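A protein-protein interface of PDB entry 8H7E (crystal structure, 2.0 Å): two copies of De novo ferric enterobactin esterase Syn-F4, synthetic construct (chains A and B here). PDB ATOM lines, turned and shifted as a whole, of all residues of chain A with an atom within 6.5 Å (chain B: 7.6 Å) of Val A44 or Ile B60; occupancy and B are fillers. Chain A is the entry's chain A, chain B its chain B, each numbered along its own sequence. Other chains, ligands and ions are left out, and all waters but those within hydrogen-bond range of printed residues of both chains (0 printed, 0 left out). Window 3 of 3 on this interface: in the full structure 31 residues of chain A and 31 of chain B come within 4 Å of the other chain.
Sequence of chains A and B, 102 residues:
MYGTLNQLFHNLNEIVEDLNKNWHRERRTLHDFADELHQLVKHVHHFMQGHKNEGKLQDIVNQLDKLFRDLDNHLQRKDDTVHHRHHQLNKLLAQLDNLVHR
Val A44 touches just one residue of chain B: Ile B60 (3.7 Å).
Of the printed residues of chain A, Leu B57 touches Phe A47 (3.5 Å).
Of the printed residues of chain B, Leu A40 touches Gln B63, Leu B64 and Leu B67.
Of the printed residues of chain B, Leu A64 touches Leu B40.
Of the printed residues of chain B, Phe A47 touches Leu B57.
The nearest residue of chain A that does not touch Ile B60 is Leu A40 (4.03 Å).
Of the 14 printed residues of chain B, 6 touch a printed residue of chain A.
Hydrophobic or aromatic side chains of chain B that line the printed part of chain A: Leu B40, Leu B57, Ile B60, Leu B64 and Leu B67.
Among the printed residues, merely in contact across the chains: Leu A40 with Gln B63 (3.6 Å), Leu A40 with Leu B64 (3.4 Å), Leu A40 with Leu B67 (3.6 Å), Val A44 with Ile B60 (3.7 Å), Phe A47 with Leu B57 (3.5 Å) and Leu A64 with Leu B40 (3.4 Å).
Leu A40 touches Leu B64, and with the chains exchanged Leu A64 touches Leu B40.
Val A44 touches Ile B60, but with the chains exchanged Ile A60 does not touch Val B44 (4.3 Å).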
ATOM      1  N   GLN A  39       4.587 -25.725   6.551  1.00  0.00           N
ATOM      2  CA  GLN A  39       4.593 -26.835   5.602  1.00  0.00           C
ATOM      3  C   GLN A  39       3.778 -26.506   4.348  1.00  0.00           C
ATOM      4  O   GLN A  39       4.272 -26.607   3.228  1.00  0.00           O
ATOM      5  CB  GLN A  39       3.995 -28.079   6.255  1.00  0.00           C
ATOM      6  CG  GLN A  39       4.820 -29.330   6.157  1.00  0.00           C
ATOM      7  CD  GLN A  39       4.098 -30.492   6.810  1.00  0.00           C
ATOM      8  OE1 GLN A  39       3.161 -31.045   6.238  1.00  0.00           O
ATOM      9  NE2 GLN A  39       4.501 -30.848   8.028  1.00  0.00           N
ATOM     10  N   LEU A  40       2.530 -26.097   4.554  1.00  0.00           N
ATOM     11  CA  LEU A  40       1.618 -25.814   3.449  1.00  0.00           C
ATOM     12  C   LEU A  40       2.101 -24.627   2.585  1.00  0.00           C
ATOM     13  O   LEU A  40       2.064 -24.708   1.362  1.00  0.00           O
ATOM     14  CB  LEU A  40       0.208 -25.604   4.000  1.00  0.00           C
ATOM     15  CG  LEU A  40      -0.971 -25.441   3.043  1.00  0.00           C
ATOM     16  CD1 LEU A  40      -1.105 -26.612   2.091  1.00  0.00           C
ATOM     17  CD2 LEU A  40      -2.240 -25.264   3.857  1.00  0.00           C
ATOM     18  N   VAL A  41       2.589 -23.565   3.229  1.00  0.00           N
ATOM     19  CA  VAL A  41       2.989 -22.320   2.549  1.00  0.00           C
ATOM     20  C   VAL A  41       4.089 -22.591   1.545  1.00  0.00           C
ATOM     21  O   VAL A  41       3.995 -22.217   0.376  1.00  0.00           O
ATOM     22  CB  VAL A  41       3.523 -21.257   3.547  1.00  0.00           C
ATOM     23  CG1 VAL A  41       4.269 -20.116   2.839  1.00  0.00           C
ATOM     24  CG2 VAL A  41       2.394 -20.689   4.394  1.00  0.00           C
ATOM     25  N   LYS A  42       5.147 -23.222   2.029  1.00  0.00           N
ATOM     26  CA  LYS A  42       6.302 -23.481   1.198  1.00  0.00           C
ATOM     27  C   LYS A  42       5.942 -24.404   0.036  1.00  0.00           C
ATOM     28  O   LYS A  42       6.367 -24.129  -1.080  1.00  0.00           O
ATOM     29  CB  LYS A  42       7.489 -23.985   2.041  1.00  0.00           C
ATOM     30  CG  LYS A  42       8.078 -22.936   3.006  1.00  0.00           C
ATOM     31  CD  LYS A  42       8.363 -21.564   2.382  1.00  0.00           C
ATOM     32  CE  LYS A  42       9.050 -20.591   3.332  1.00  0.00           C
ATOM     33  NZ  LYS A  42      10.534 -20.556   3.209  1.00  0.00           N
ATOM     34  N   HIS A  43       5.116 -25.432   0.265  1.00  0.00           N
ATOM     35  CA  HIS A  43       4.672 -26.314  -0.836  1.00  0.00           C
ATOM     36  C   HIS A  43       3.880 -25.541  -1.894  1.00  0.00           C
ATOM     37  O   HIS A  43       4.200 -25.585  -3.080  1.00  0.00           O
ATOM     38  CB  HIS A  43       3.848 -27.494  -0.327  1.00  0.00           C
ATOM     39  CG  HIS A  43       4.620 -28.432   0.545  1.00  0.00           C
ATOM     40  ND1 HIS A  43       4.019 -29.246   1.481  1.00  0.00           N
ATOM     41  CD2 HIS A  43       5.952 -28.670   0.641  1.00  0.00           C
ATOM     42  CE1 HIS A  43       4.944 -29.955   2.105  1.00  0.00           C
ATOM     43  NE2 HIS A  43       6.126 -29.622   1.616  1.00  0.00           N
ATOM     44  N   VAL A  44       2.870 -24.803  -1.452  1.00  0.00           N
ATOM     45  CA  VAL A  44       2.129 -23.902  -2.344  1.00  0.00           C
ATOM     46  C   VAL A  44       3.103 -22.976  -3.111  1.00  0.00           C
ATOM     47  O   VAL A  44       2.979 -22.834  -4.328  1.00  0.00           O
ATOM     48  CB  VAL A  44       1.050 -23.109  -1.563  1.00  0.00           C
ATOM     49  CG1 VAL A  44       0.520 -21.926  -2.360  1.00  0.00           C
ATOM     50  CG2 VAL A  44      -0.101 -24.029  -1.168  1.00  0.00           C
ATOM     51  N   HIS A  45       4.077 -22.392  -2.405  1.00  0.00           N
ATOM     52  CA  HIS A  45       5.110 -21.544  -3.026  1.00  0.00           C
ATOM     53  C   HIS A  45       6.052 -22.299  -3.985  1.00  0.00           C
ATOM     54  O   HIS A  45       6.534 -21.705  -4.955  1.00  0.00           O
ATOM     55  CB  HIS A  45       5.925 -20.798  -1.958  1.00  0.00           C
ATOM     56  CG  HIS A  45       6.885 -19.793  -2.523  1.00  0.00           C
ATOM     57  ND1 HIS A  45       8.238 -19.822  -2.255  1.00  0.00           N
ATOM     58  CD2 HIS A  45       6.691 -18.748  -3.364  1.00  0.00           C
ATOM     59  CE1 HIS A  45       8.834 -18.830  -2.895  1.00  0.00           C
ATOM     60  NE2 HIS A  45       7.918 -18.165  -3.576  1.00  0.00           N
ATOM     61  N   HIS A  46       6.327 -23.581  -3.715  1.00  0.00           N
ATOM     62  CA  HIS A  46       7.070 -24.433  -4.662  1.00  0.00           C
ATOM     63  C   HIS A  46       6.256 -24.544  -5.947  1.00  0.00           C
ATOM     64  O   HIS A  46       6.711 -24.161  -7.024  1.00  0.00           O
ATOM     65  CB  HIS A  46       7.311 -25.863  -4.139  1.00  0.00           C
ATOM     66  CG  HIS A  46       8.191 -25.956  -2.928  1.00  0.00           C
ATOM     67  ND1 HIS A  46       8.263 -27.101  -2.159  1.00  0.00           N
ATOM     68  CD2 HIS A  46       9.026 -25.061  -2.348  1.00  0.00           C
ATOM     69  CE1 HIS A  46       9.107 -26.907  -1.163  1.00  0.00           C
ATOM     70  NE2 HIS A  46       9.582 -25.677  -1.252  1.00  0.00           N
ATOM     71  N   PHE A  47       5.038 -25.054  -5.789  1.00  0.00           N
ATOM     72  CA  PHE A  47       4.132 -25.378  -6.887  1.00  0.00           C
ATOM     73  C   PHE A  47       3.945 -24.204  -7.859  1.00  0.00           C
ATOM     74  O   PHE A  47       4.071 -24.376  -9.077  1.00  0.00           O
ATOM     75  CB  PHE A  47       2.790 -25.841  -6.293  1.00  0.00           C
ATOM     76  CG  PHE A  47       1.689 -25.986  -7.297  1.00  0.00           C
ATOM     77  CD1 PHE A  47       0.852 -24.906  -7.586  1.00  0.00           C
ATOM     78  CD2 PHE A  47       1.473 -27.196  -7.941  1.00  0.00           C
ATOM     79  CE1 PHE A  47      -0.171 -25.028  -8.512  1.00  0.00           C
ATOM     80  CE2 PHE A  47       0.448 -27.327  -8.867  1.00  0.00           C
ATOM     81  CZ  PHE A  47      -0.375 -26.241  -9.153  1.00  0.00           C
ATOM     82  N   MET A  48       3.661 -23.024  -7.309  1.00  0.00           N
ATOM     83  CA  MET A  48       3.486 -21.805  -8.106  1.00  0.00           C
ATOM     84  C   MET A  48       4.726 -21.494  -8.951  1.00  0.00           C
ATOM     85  O   MET A  48       5.857 -21.653  -8.495  1.00  0.00           O
ATOM     86  CB  MET A  48       3.169 -20.610  -7.194  1.00  0.00           C
ATOM     87  CG  MET A  48       2.887 -19.310  -7.938  1.00  0.00           C
ATOM     88  SD  MET A  48       2.599 -17.899  -6.859  1.00  0.00           S
ATOM     89  CE  MET A  48       4.247 -17.544  -6.251  1.00  0.00           C
ATOM     90  N   ILE A  60      -3.128 -16.512  -3.581  1.00  0.00           N
ATOM     91  CA  ILE A  60      -3.164 -17.575  -2.563  1.00  0.00           C
ATOM     92  C   ILE A  60      -1.878 -17.644  -1.714  1.00  0.00           C
ATOM     93  O   ILE A  60      -1.950 -17.848  -0.498  1.00  0.00           O
ATOM     94  CB  ILE A  60      -3.497 -18.948  -3.204  1.00  0.00           C
ATOM     95  CG1 ILE A  60      -4.934 -18.939  -3.743  1.00  0.00           C
ATOM     96  CG2 ILE A  60      -3.351 -20.085  -2.200  1.00  0.00           C
ATOM     97  CD1 ILE A  60      -5.207 -19.971  -4.818  1.00  0.00           C
ATOM     98  N   VAL A  61      -0.719 -17.473  -2.350  1.00  0.00           N
ATOM     99  CA  VAL A  61       0.570 -17.452  -1.640  1.00  0.00           C
ATOM    100  C   VAL A  61       0.619 -16.323  -0.596  1.00  0.00           C
ATOM    101  O   VAL A  61       0.953 -16.560   0.566  1.00  0.00           O
ATOM    102  CB  VAL A  61       1.762 -17.317  -2.623  1.00  0.00           C
ATOM    103  CG1 VAL A  61       3.071 -17.031  -1.892  1.00  0.00           C
ATOM    104  CG2 VAL A  61       1.907 -18.589  -3.440  1.00  0.00           C
ATOM    105  N   LEU A  64      -1.669 -17.021   2.406  1.00  0.00           N
ATOM    106  CA  LEU A  64      -1.099 -18.023   3.325  1.00  0.00           C
ATOM    107  C   LEU A  64       0.065 -17.494   4.125  1.00  0.00           C
ATOM    108  O   LEU A  64       0.191 -17.751   5.317  1.00  0.00           O
ATOM    109  CB  LEU A  64      -0.600 -19.249   2.566  1.00  0.00           C
ATOM    110  CG  LEU A  64      -1.620 -20.325   2.250  1.00  0.00           C
ATOM    111  CD1 LEU A  64      -1.098 -21.262   1.171  1.00  0.00           C
ATOM    112  CD2 LEU A  64      -2.017 -21.082   3.505  1.00  0.00           C
ATOM    113  N   LEU B  40      -9.827 -19.387   1.882  1.00  0.00           N
ATOM    114  CA  LEU B  40      -8.720 -19.980   1.122  1.00  0.00           C
ATOM    115  C   LEU B  40      -9.038 -21.340   0.505  1.00  0.00           C
ATOM    116  O   LEU B  40      -8.604 -21.627  -0.610  1.00  0.00           O
ATOM    117  CB  LEU B  40      -7.494 -20.118   2.038  1.00  0.00           C
ATOM    118  CG  LEU B  40      -6.101 -19.882   1.461  1.00  0.00           C
ATOM    119  CD1 LEU B  40      -6.032 -18.596   0.646  1.00  0.00           C
ATOM    120  CD2 LEU B  40      -5.109 -19.861   2.615  1.00  0.00           C
ATOM    121  N   VAL B  41      -9.787 -22.158   1.244  1.00  0.00           N
ATOM    122  CA  VAL B  41     -10.294 -23.450   0.764  1.00  0.00           C
ATOM    123  C   VAL B  41     -11.132 -23.296  -0.517  1.00  0.00           C
ATOM    124  O   VAL B  41     -11.000 -24.090  -1.455  1.00  0.00           O
ATOM    125  CB  VAL B  41     -11.143 -24.157   1.860  1.00  0.00           C
ATOM    126  CG1 VAL B  41     -11.903 -25.362   1.306  1.00  0.00           C
ATOM    127  CG2 VAL B  41     -10.273 -24.595   3.035  1.00  0.00           C
ATOM    128  N   VAL B  44      -8.904 -21.920  -3.484  1.00  0.00           N
ATOM    129  CA  VAL B  44      -8.173 -23.055  -4.053  1.00  0.00           C
ATOM    130  C   VAL B  44      -9.101 -23.876  -4.953  1.00  0.00           C
ATOM    131  O   VAL B  44      -8.861 -23.970  -6.161  1.00  0.00           O
ATOM    132  CB  VAL B  44      -7.531 -23.947  -2.956  1.00  0.00           C
ATOM    133  CG1 VAL B  44      -7.054 -25.284  -3.517  1.00  0.00           C
ATOM    134  CG2 VAL B  44      -6.361 -23.220  -2.315  1.00  0.00           C
ATOM    135  N   LEU B  57      -2.956 -29.851  -6.997  1.00  0.00           N
ATOM    136  CA  LEU B  57      -3.416 -29.036  -5.878  1.00  0.00           C
ATOM    137  C   LEU B  57      -4.376 -29.796  -4.955  1.00  0.00           C
ATOM    138  O   LEU B  57      -5.194 -29.177  -4.260  1.00  0.00           O
ATOM    139  CB  LEU B  57      -4.100 -27.772  -6.406  1.00  0.00           C
ATOM    140  CG  LEU B  57      -3.312 -26.975  -7.456  1.00  0.00           C
ATOM    141  CD1 LEU B  57      -3.769 -27.327  -8.866  1.00  0.00           C
ATOM    142  CD2 LEU B  57      -3.440 -25.475  -7.226  1.00  0.00           C
ATOM    143  N   GLN B  58      -4.263 -31.125  -4.936  1.00  0.00           N
ATOM    144  CA  GLN B  58      -5.227 -31.975  -4.230  1.00  0.00           C
ATOM    145  C   GLN B  58      -4.769 -32.218  -2.796  1.00  0.00           C
ATOM    146  O   GLN B  58      -5.579 -32.139  -1.871  1.00  0.00           O
ATOM    147  CB  GLN B  58      -5.450 -33.295  -4.989  1.00  0.00           C
ATOM    148  CG  GLN B  58      -6.591 -34.175  -4.469  1.00  0.00           C
ATOM    149  CD  GLN B  58      -7.936 -33.455  -4.355  1.00  0.00           C
ATOM    150  OE1 GLN B  58      -8.186 -32.456  -5.031  1.00  0.00           O
ATOM    151  NE2 GLN B  58      -8.811 -33.969  -3.490  1.00  0.00           N
ATOM    152  N   ASP B  59      -3.479 -32.522  -2.626  1.00  0.00           N
ATOM    153  CA  ASP B  59      -2.802 -32.395  -1.326  1.00  0.00           C
ATOM    154  C   ASP B  59      -3.179 -31.081  -0.606  1.00  0.00           C
ATOM    155  O   ASP B  59      -3.600 -31.098   0.550  1.00  0.00           O
ATOM    156  CB  ASP B  59      -1.269 -32.460  -1.503  1.00  0.00           C
ATOM    157  CG  ASP B  59      -0.732 -33.893  -1.551  1.00  0.00           C
ATOM    158  OD1 ASP B  59      -0.798 -34.593  -0.512  1.00  0.00           O
ATOM    159  OD2 ASP B  59      -0.224 -34.310  -2.619  1.00  0.00           O
ATOM    160  N   ILE B  60      -3.043 -29.967  -1.325  1.00  0.00           N
ATOM    161  CA  ILE B  60      -3.195 -28.606  -0.775  1.00  0.00           C
ATOM    162  C   ILE B  60      -4.584 -28.295  -0.222  1.00  0.00           C
ATOM    163  O   ILE B  60      -4.716 -27.992   0.966  1.00  0.00           O
ATOM    164  CB  ILE B  60      -2.770 -27.539  -1.813  1.00  0.00           C
ATOM    165  CG1 ILE B  60      -1.242 -27.531  -1.935  1.00  0.00           C
ATOM    166  CG2 ILE B  60      -3.271 -26.140  -1.437  1.00  0.00           C
ATOM    167  CD1 ILE B  60      -0.732 -26.994  -3.250  1.00  0.00           C
ATOM    168  N   VAL B  61      -5.603 -28.350  -1.076  1.00  0.00           N
ATOM    169  CA  VAL B  61      -6.991 -28.140  -0.632  1.00  0.00           C
ATOM    170  C   VAL B  61      -7.340 -28.988   0.609  1.00  0.00           C
ATOM    171  O   VAL B  61      -7.993 -28.484   1.529  1.00  0.00           O
ATOM    172  CB  VAL B  61      -8.010 -28.371  -1.776  1.00  0.00           C
ATOM    173  CG1 VAL B  61      -8.062 -29.832  -2.202  1.00  0.00           C
ATOM    174  CG2 VAL B  61      -9.395 -27.867  -1.385  1.00  0.00           C
ATOM    175  N   ASN B  62      -6.876 -30.243   0.644  1.00  0.00           N
ATOM    176  CA  ASN B  62      -7.129 -31.150   1.774  1.00  0.00           C
ATOM    177  C   ASN B  62      -6.402 -30.724   3.037  1.00  0.00           C
ATOM    178  O   ASN B  62      -6.912 -30.917   4.139  1.00  0.00           O
ATOM    179  CB  ASN B  62      -6.703 -32.587   1.456  1.00  0.00           C
ATOM    180  CG  ASN B  62      -7.480 -33.204   0.302  1.00  0.00           C
ATOM    181  OD1 ASN B  62      -8.544 -32.718  -0.096  1.00  0.00           O
ATOM    182  ND2 ASN B  62      -6.934 -34.286  -0.250  1.00  0.00           N
ATOM    183  N   GLN B  63      -5.197 -30.181   2.874  1.00  0.00           N
ATOM    184  CA  GLN B  63      -4.414 -29.698   4.006  1.00  0.00           C
ATOM    185  C   GLN B  63      -5.083 -28.494   4.651  1.00  0.00           C
ATOM    186  O   GLN B  63      -5.135 -28.409   5.873  1.00  0.00           O
ATOM    187  CB  GLN B  63      -2.975 -29.349   3.588  1.00  0.00           C
ATOM    188  CG  GLN B  63      -2.010 -29.115   4.751  1.00  0.00           C
ATOM    189  CD  GLN B  63      -1.874 -30.313   5.684  1.00  0.00           C
ATOM    190  OE1 GLN B  63      -2.037 -31.465   5.263  1.00  0.00           O
ATOM    191  NE2 GLN B  63      -1.585 -30.051   6.960  1.00  0.00           N
ATOM    192  N   LEU B  64      -5.588 -27.577   3.828  1.00  0.00           N
ATOM    193  CA  LEU B  64      -6.319 -26.409   4.324  1.00  0.00           C
ATOM    194  C   LEU B  64      -7.537 -26.795   5.156  1.00  0.00           C
ATOM    195  O   LEU B  64      -7.750 -26.243   6.230  1.00  0.00           O
ATOM    196  CB  LEU B  64      -6.742 -25.487   3.175  1.00  0.00           C
ATOM    197  CG  LEU B  64      -5.670 -24.603   2.564  1.00  0.00           C
ATOM    198  CD1 LEU B  64      -6.220 -23.874   1.346  1.00  0.00           C
ATOM    199  CD2 LEU B  64      -5.168 -23.592   3.576  1.00  0.00           C
ATOM    200  N   ASP B  65      -8.323 -27.743   4.658  1.00  0.00           N
ATOM    201  CA  ASP B  65      -9.454 -28.310   5.396  1.00  0.00           C
ATOM    202  C   ASP B  65      -9.057 -28.833   6.765  1.00  0.00           C
ATOM    203  O   ASP B  65      -9.672 -28.503   7.771  1.00  0.00           O
ATOM    204  CB  ASP B  65     -10.062 -29.494   4.626  1.00  0.00           C
ATOM    205  CG  ASP B  65     -10.943 -29.064   3.487  1.00  0.00           C
ATOM    206  OD1 ASP B  65     -11.826 -28.203   3.698  1.00  0.00           O
ATOM    207  OD2 ASP B  65     -10.772 -29.614   2.381  1.00  0.00           O
ATOM    208  N   LYS B  66      -8.041 -29.681   6.776  1.00  0.00           N
ATOM    209  CA  LYS B  66      -7.512 -30.255   8.006  1.00  0.00           C
ATOM    210  C   LYS B  66      -7.146 -29.163   9.011  1.00  0.00           C
ATOM    211  O   LYS B  66      -7.566 -29.210  10.172  1.00  0.00           O
ATOM    212  CB  LYS B  66      -6.269 -31.092   7.722  1.00  0.00           C
ATOM    213  CG  LYS B  66      -5.919 -32.033   8.865  1.00  0.00           C
ATOM    214  CD  LYS B  66      -4.456 -31.961   9.246  1.00  0.00           C
ATOM    215  CE  LYS B  66      -4.251 -32.569  10.618  1.00  0.00           C
ATOM    216  NZ  LYS B  66      -3.051 -32.036  11.318  1.00  0.00           N
ATOM    217  N   LEU B  67      -6.370 -28.189   8.545  1.00  0.00           N
ATOM    218  CA  LEU B  67      -5.965 -27.080   9.394  1.00  0.00           C
ATOM    219  C   LEU B  67      -7.193 -26.341   9.886  1.00  0.00           C
ATOM    220  O   LEU B  67      -7.321 -26.081  11.087  1.00  0.00           O
ATOM    221  CB  LEU B  67      -5.009 -26.142   8.662  1.00  0.00           C
ATOM    222  CG  LEU B  67      -3.582 -26.677   8.426  1.00  0.00           C
ATOM    223  CD1 LEU B  67      -2.856 -25.911   7.335  1.00  0.00           C
ATOM    224  CD2 LEU B  67      -2.758 -26.581   9.693  1.00  0.00           C
